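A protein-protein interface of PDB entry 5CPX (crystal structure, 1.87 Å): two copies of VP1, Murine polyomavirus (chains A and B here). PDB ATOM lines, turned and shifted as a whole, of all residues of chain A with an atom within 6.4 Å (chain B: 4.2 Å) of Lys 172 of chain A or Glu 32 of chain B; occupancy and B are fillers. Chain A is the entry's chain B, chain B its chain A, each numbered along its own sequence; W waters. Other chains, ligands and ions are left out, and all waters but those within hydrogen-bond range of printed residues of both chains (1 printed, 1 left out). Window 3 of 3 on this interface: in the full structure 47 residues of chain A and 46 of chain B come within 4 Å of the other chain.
No position is printed for both chains.
Of the 6 pairs that touch across the chains among the printed residues, none has its exchanged pair printed and touching as well.
The backbone NH of Gly 38 of chain B sits close to the backbone carbonyl oxygen of Pro 31 of chain B (3.4 Å).
The backbone carbonyl oxygen of Ser 33 of chain B is in hydrogen-bond range of the backbone NH of Gly 38 of chain B (2.9 Å).
O of Pro 29 of chain B lies within hydrogen-bond range of ND2 of Asn 171 of chain A, at 3.0 Å.
NZ of Lys 172 of chain A lies within salt-bridge range of OE2 of Glu 32 of chain B (3.6 Å).
Water W1 lies within hydrogen-bond range of the backbone carbonyl oxygen of Glu 32 of chain B (2.7 Å) and the backbone NH of Asn 171 of chain A (2.9 Å).
Of the 12 printed residues of chain A, 2 touch a printed residue of chain B.
Hydrophobic or aromatic side chains of chain B within 4 Å of the printed part of chain A: Leu 34.
Among the printed residues, 6 pairs touch across the chains.
Among the printed residues, Asp or Glu carboxylates within 4 Å of a Lys or Arg side-chain nitrogen of the other chain: Lys 172 of chain A with Glu 32 of chain B.
Of the printed residues of chain A, Pro 29 of chain B touches Asn 171 (3.0 Å).
Of the printed residues of chain A, Pro 31 of chain B touches Asn 171 (3.8 Å).
Glu 32 of chain B touches just these residues of chain A: Asn 171 and Lys 172.
Of the printed residues of chain A, Leu 34 of chain B touches Asn 171 (3.7 Å).
Of the printed residues of chain A, Gly 38 of chain B touches Asn 171.
The nearest printed residue of chain B that does not touch Lys 172 of chain A is Pro 29 of chain B (6.1 Å).
The nearest residue of chain A that does not touch Glu 32 of chain B is Val 170 of chain A (5.6 Å).
The nearest printed residue of chain A that does not touch Leu 34 of chain B is Ala 149 of chain A (4.1 Å).
Among the printed residues, pairs that only touch across the chains: Asn 171 of chain A with Gly 38 of chain B, Asn 171 of chain A with Glu 32 of chain B, Asn 171 of chain A with Leu 34 of chain B and Asn 171 of chain A with Pro 31 of chain B.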
ATOM      1  N   GLY A 144      -3.300  15.236 -21.658  1.00  0.00           N
ATOM      2  CA  GLY A 144      -2.170  15.941 -22.271  1.00  0.00           C
ATOM      3  C   GLY A 144      -1.950  17.269 -21.568  1.00  0.00           C
ATOM      4  O   GLY A 144      -2.918  17.940 -21.202  1.00  0.00           O
ATOM      5  N   LEU A 145      -0.683  17.608 -21.309  1.00  0.00           N
ATOM      6  CA  LEU A 145      -0.287  18.932 -20.804  1.00  0.00           C
ATOM      7  C   LEU A 145       1.201  19.096 -21.083  1.00  0.00           C
ATOM      8  O   LEU A 145       1.997  18.254 -20.669  1.00  0.00           O
ATOM      9  CB  LEU A 145      -0.561  19.107 -19.292  1.00  0.00           C
ATOM     10  CG  LEU A 145      -0.363  20.521 -18.714  1.00  0.00           C
ATOM     11  CD1 LEU A 145      -1.279  20.737 -17.506  1.00  0.00           C
ATOM     12  CD2 LEU A 145       1.080  20.817 -18.309  1.00  0.00           C
ATOM     13  N   ALA A 149       3.458  24.562 -26.200  1.00  0.00           N
ATOM     14  CA  ALA A 149       2.533  24.113 -27.242  1.00  0.00           C
ATOM     15  C   ALA A 149       3.127  24.292 -28.642  1.00  0.00           C
ATOM     16  O   ALA A 149       2.531  23.853 -29.633  1.00  0.00           O
ATOM     17  CB  ALA A 149       1.208  24.867 -27.143  1.00  0.00           C
ATOM     18  N   VAL A 170      -2.698  23.911 -29.096  1.00  0.00           N
ATOM     19  CA  VAL A 170      -3.167  25.284 -28.837  1.00  0.00           C
ATOM     20  C   VAL A 170      -2.594  25.756 -27.491  1.00  0.00           C
ATOM     21  O   VAL A 170      -2.084  24.936 -26.721  1.00  0.00           O
ATOM     22  CB  VAL A 170      -4.716  25.361 -28.821  1.00  0.00           C
ATOM     23  CG1 VAL A 170      -5.284  25.126 -30.222  1.00  0.00           C
ATOM     24  CG2 VAL A 170      -5.314  24.362 -27.825  1.00  0.00           C
ATOM     25  N   ASN A 171      -2.676  27.055 -27.198  1.00  0.00           N
ATOM     26  CA  ASN A 171      -2.095  27.555 -25.946  1.00  0.00           C
ATOM     27  C   ASN A 171      -2.674  26.899 -24.693  1.00  0.00           C
ATOM     28  O   ASN A 171      -1.960  26.719 -23.702  1.00  0.00           O
ATOM     29  CB  ASN A 171      -2.086  29.096 -25.866  1.00  0.00           C
ATOM     30  CG  ASN A 171      -3.434  29.709 -25.506  1.00  0.00           C
ATOM     31  OD1 ASN A 171      -4.510  29.174 -25.827  1.00  0.00           O
ATOM     32  ND2 ASN A 171      -3.379  30.875 -24.855  1.00  0.00           N
ATOM     33  N   LYS A 172      -3.947  26.508 -24.757  1.00  0.00           N
ATOM     34  CA  LYS A 172      -4.606  25.805 -23.641  1.00  0.00           C
ATOM     35  C   LYS A 172      -3.929  24.486 -23.282  1.00  0.00           C
ATOM     36  O   LYS A 172      -4.137  23.968 -22.185  1.00  0.00           O
ATOM     37  CB  LYS A 172      -6.078  25.509 -23.955  1.00  0.00           C
ATOM     38  CG  LYS A 172      -6.921  26.729 -24.272  1.00  0.00           C
ATOM     39  CD  LYS A 172      -8.309  26.320 -24.742  1.00  0.00           C
ATOM     40  CE  LYS A 172      -8.921  27.414 -25.602  1.00  0.00           C
ATOM     41  NZ  LYS A 172     -10.328  27.120 -25.983  1.00  0.00           N
ATOM     42  N   ASP A 173      -3.138  23.936 -24.204  1.00  0.00           N
ATOM     43  CA  ASP A 173      -2.396  22.695 -23.938  1.00  0.00           C
ATOM     44  C   ASP A 173      -1.239  22.860 -22.951  1.00  0.00           C
ATOM     45  O   ASP A 173      -0.673  21.866 -22.482  1.00  0.00           O
ATOM     46  CB  ASP A 173      -1.948  22.025 -25.253  1.00  0.00           C
ATOM     47  CG  ASP A 173      -3.137  21.526 -26.085  1.00  0.00           C
ATOM     48  OD1 ASP A 173      -4.137  21.058 -25.488  1.00  0.00           O
ATOM     49  OD2 ASP A 173      -3.083  21.606 -27.335  1.00  0.00           O
ATOM     50  N   GLN A 174      -0.900  24.108 -22.623  1.00  0.00           N
ATOM     51  CA  GLN A 174       0.098  24.389 -21.580  1.00  0.00           C
ATOM     52  C   GLN A 174      -0.526  24.416 -20.187  1.00  0.00           C
ATOM     53  O   GLN A 174       0.185  24.481 -19.186  1.00  0.00           O
ATOM     54  CB  GLN A 174       0.848  25.696 -21.880  1.00  0.00           C
ATOM     55  CG  GLN A 174       1.675  25.557 -23.153  1.00  0.00           C
ATOM     56  CD  GLN A 174       2.397  26.816 -23.601  1.00  0.00           C
ATOM     57  OE1 GLN A 174       3.020  26.813 -24.661  1.00  0.00           O
ATOM     58  NE2 GLN A 174       2.325  27.890 -22.808  1.00  0.00           N
ATOM     59  N   VAL A 175      -1.860  24.383 -20.138  1.00  0.00           N
ATOM     60  CA  VAL A 175      -2.613  24.219 -18.886  1.00  0.00           C
ATOM     61  C   VAL A 175      -3.546  23.006 -19.095  1.00  0.00           C
ATOM     62  O   VAL A 175      -3.225  22.129 -19.880  1.00  0.00           O
ATOM     63  CB  VAL A 175      -3.400  25.501 -18.480  1.00  0.00           C
ATOM     64  CG1 VAL A 175      -2.449  26.651 -18.188  1.00  0.00           C
ATOM     65  CG2 VAL A 175      -4.409  25.922 -19.539  1.00  0.00           C
ATOM     66  N   LEU A 176      -4.692  22.962 -18.422  1.00  0.00           N
ATOM     67  CA  LEU A 176      -5.618  21.838 -18.617  1.00  0.00           C
ATOM     68  C   LEU A 176      -6.619  22.118 -19.746  1.00  0.00           C
ATOM     69  O   LEU A 176      -7.492  22.983 -19.606  1.00  0.00           O
ATOM     70  CB  LEU A 176      -6.356  21.521 -17.300  1.00  0.00           C
ATOM     71  CG  LEU A 176      -6.947  20.108 -17.103  1.00  0.00           C
ATOM     72  CD1 LEU A 176      -7.980  19.723 -18.168  1.00  0.00           C
ATOM     73  CD2 LEU A 176      -5.835  19.079 -17.033  1.00  0.00           C
ATOM     74  N   ASN A 177      -6.484  21.372 -20.845  1.00  0.00           N
ATOM     75  CA  ASN A 177      -7.399  21.413 -21.975  1.00  0.00           C
ATOM     76  C   ASN A 177      -8.083  20.024 -22.064  1.00  0.00           C
ATOM     77  O   ASN A 177      -7.434  19.043 -22.457  1.00  0.00           O
ATOM     78  CB  ASN A 177      -6.640  21.757 -23.271  1.00  0.00           C
ATOM     79  CG  ASN A 177      -7.531  21.730 -24.505  1.00  0.00           C
ATOM     80  OD1 ASN A 177      -8.749  21.592 -24.399  1.00  0.00           O
ATOM     81  ND2 ASN A 177      -6.928  21.855 -25.684  1.00  0.00           N
ATOM     82  N   ILE A 179      -9.949  18.641 -24.080  1.00  0.00           N
ATOM     83  CA  ILE A 179      -9.934  18.022 -25.411  1.00  0.00           C
ATOM     84  C   ILE A 179      -8.748  17.062 -25.600  1.00  0.00           C
ATOM     85  O   ILE A 179      -8.846  16.070 -26.324  1.00  0.00           O
ATOM     86  CB  ILE A 179      -9.928  19.099 -26.526  1.00  0.00           C
ATOM     87  CG1 ILE A 179     -11.274  19.832 -26.559  1.00  0.00           C
ATOM     88  CG2 ILE A 179      -9.618  18.499 -27.893  1.00  0.00           C
ATOM     89  CD1 ILE A 179     -11.270  21.076 -27.432  1.00  0.00           C
ATOM     90  N   PRO B  29      -5.674  33.880 -20.423  1.00  0.00           N
ATOM     91  CA  PRO B  29      -5.948  32.848 -21.438  1.00  0.00           C
ATOM     92  C   PRO B  29      -5.957  33.372 -22.881  1.00  0.00           C
ATOM     93  O   PRO B  29      -5.640  32.629 -23.809  1.00  0.00           O
ATOM     94  CB  PRO B  29      -7.338  32.330 -21.038  1.00  0.00           C
ATOM     95  CG  PRO B  29      -7.399  32.579 -19.560  1.00  0.00           C
ATOM     96  CD  PRO B  29      -6.752  33.933 -19.417  1.00  0.00           C
ATOM     97  N   THR B  30      -6.312  34.640 -23.072  1.00  0.00           N
ATOM     98  CA  THR B  30      -6.307  35.236 -24.408  1.00  0.00           C
ATOM     99  C   THR B  30      -5.309  36.407 -24.418  1.00  0.00           C
ATOM    100  O   THR B  30      -5.054  36.977 -23.363  1.00  0.00           O
ATOM    101  CB  THR B  30      -7.723  35.701 -24.824  1.00  0.00           C
ATOM    102  OG1 THR B  30      -8.128  36.787 -23.989  1.00  0.00           O
ATOM    103  CG2 THR B  30      -8.732  34.557 -24.677  1.00  0.00           C
ATOM    104  N   PRO B  31      -4.711  36.745 -25.583  1.00  0.00           N
ATOM    105  CA  PRO B  31      -4.901  36.154 -26.920  1.00  0.00           C
ATOM    106  C   PRO B  31      -4.386  34.720 -27.001  1.00  0.00           C
ATOM    107  O   PRO B  31      -3.376  34.381 -26.381  1.00  0.00           O
ATOM    108  CB  PRO B  31      -4.098  37.075 -27.850  1.00  0.00           C
ATOM    109  CG  PRO B  31      -3.112  37.757 -26.979  1.00  0.00           C
ATOM    110  CD  PRO B  31      -3.660  37.783 -25.582  1.00  0.00           C
ATOM    111  N   GLU B  32      -5.094  33.888 -27.754  1.00  0.00           N
ATOM    112  CA  GLU B  32      -4.724  32.482 -27.899  1.00  0.00           C
ATOM    113  C   GLU B  32      -3.486  32.267 -28.769  1.00  0.00           C
ATOM    114  O   GLU B  32      -2.795  31.268 -28.612  1.00  0.00           O
ATOM    115  CB  GLU B  32      -5.916  31.673 -28.436  1.00  0.00           C
ATOM    116  CG  GLU B  32      -7.039  31.556 -27.412  1.00  0.00           C
ATOM    117  CD  GLU B  32      -8.268  30.808 -27.915  1.00  0.00           C
ATOM    118  OE1 GLU B  32      -8.454  30.675 -29.148  1.00  0.00           O
ATOM    119  OE2 GLU B  32      -9.062  30.360 -27.058  1.00  0.00           O
ATOM    120  N   SER B  33      -3.207  33.210 -29.668  1.00  0.00           N
ATOM    121  CA  SER B  33      -2.115  33.074 -30.624  1.00  0.00           C
ATOM    122  C   SER B  33      -0.766  32.771 -29.970  1.00  0.00           C
ATOM    123  O   SER B  33      -0.343  33.448 -29.025  1.00  0.00           O
ATOM    124  CB  SER B  33      -1.991  34.335 -31.481  1.00  0.00           C
ATOM    125  OG  SER B  33      -0.745  34.350 -32.143  1.00  0.00           O
ATOM    126  N   LEU B  34      -0.083  31.764 -30.507  1.00  0.00           N
ATOM    127  CA  LEU B  34       1.219  31.349 -29.965  1.00  0.00           C
ATOM    128  C   LEU B  34       2.366  32.275 -30.383  1.00  0.00           C
ATOM    129  O   LEU B  34       3.531  32.036 -30.037  1.00  0.00           O
ATOM    130  CB  LEU B  34       1.504  29.884 -30.323  1.00  0.00           C
ATOM    131  CG  LEU B  34       0.572  28.850 -29.678  1.00  0.00           C
ATOM    132  CD1 LEU B  34       0.775  27.478 -30.313  1.00  0.00           C
ATOM    133  CD2 LEU B  34       0.767  28.778 -28.163  1.00  0.00           C
ATOM    134  N   GLY B  38       0.044  34.204 -26.281  1.00  0.00           N
ATOM    135  CA  GLY B  38      -0.551  32.941 -25.829  1.00  0.00           C
ATOM    136  C   GLY B  38       0.460  31.861 -25.499  1.00  0.00           C
ATOM    137  O   GLY B  38       0.179  30.975 -24.705  1.00  0.00           O
HETATM  138  O   HOH W   1      -3.651  28.811 -29.273  1.00  0.00           O
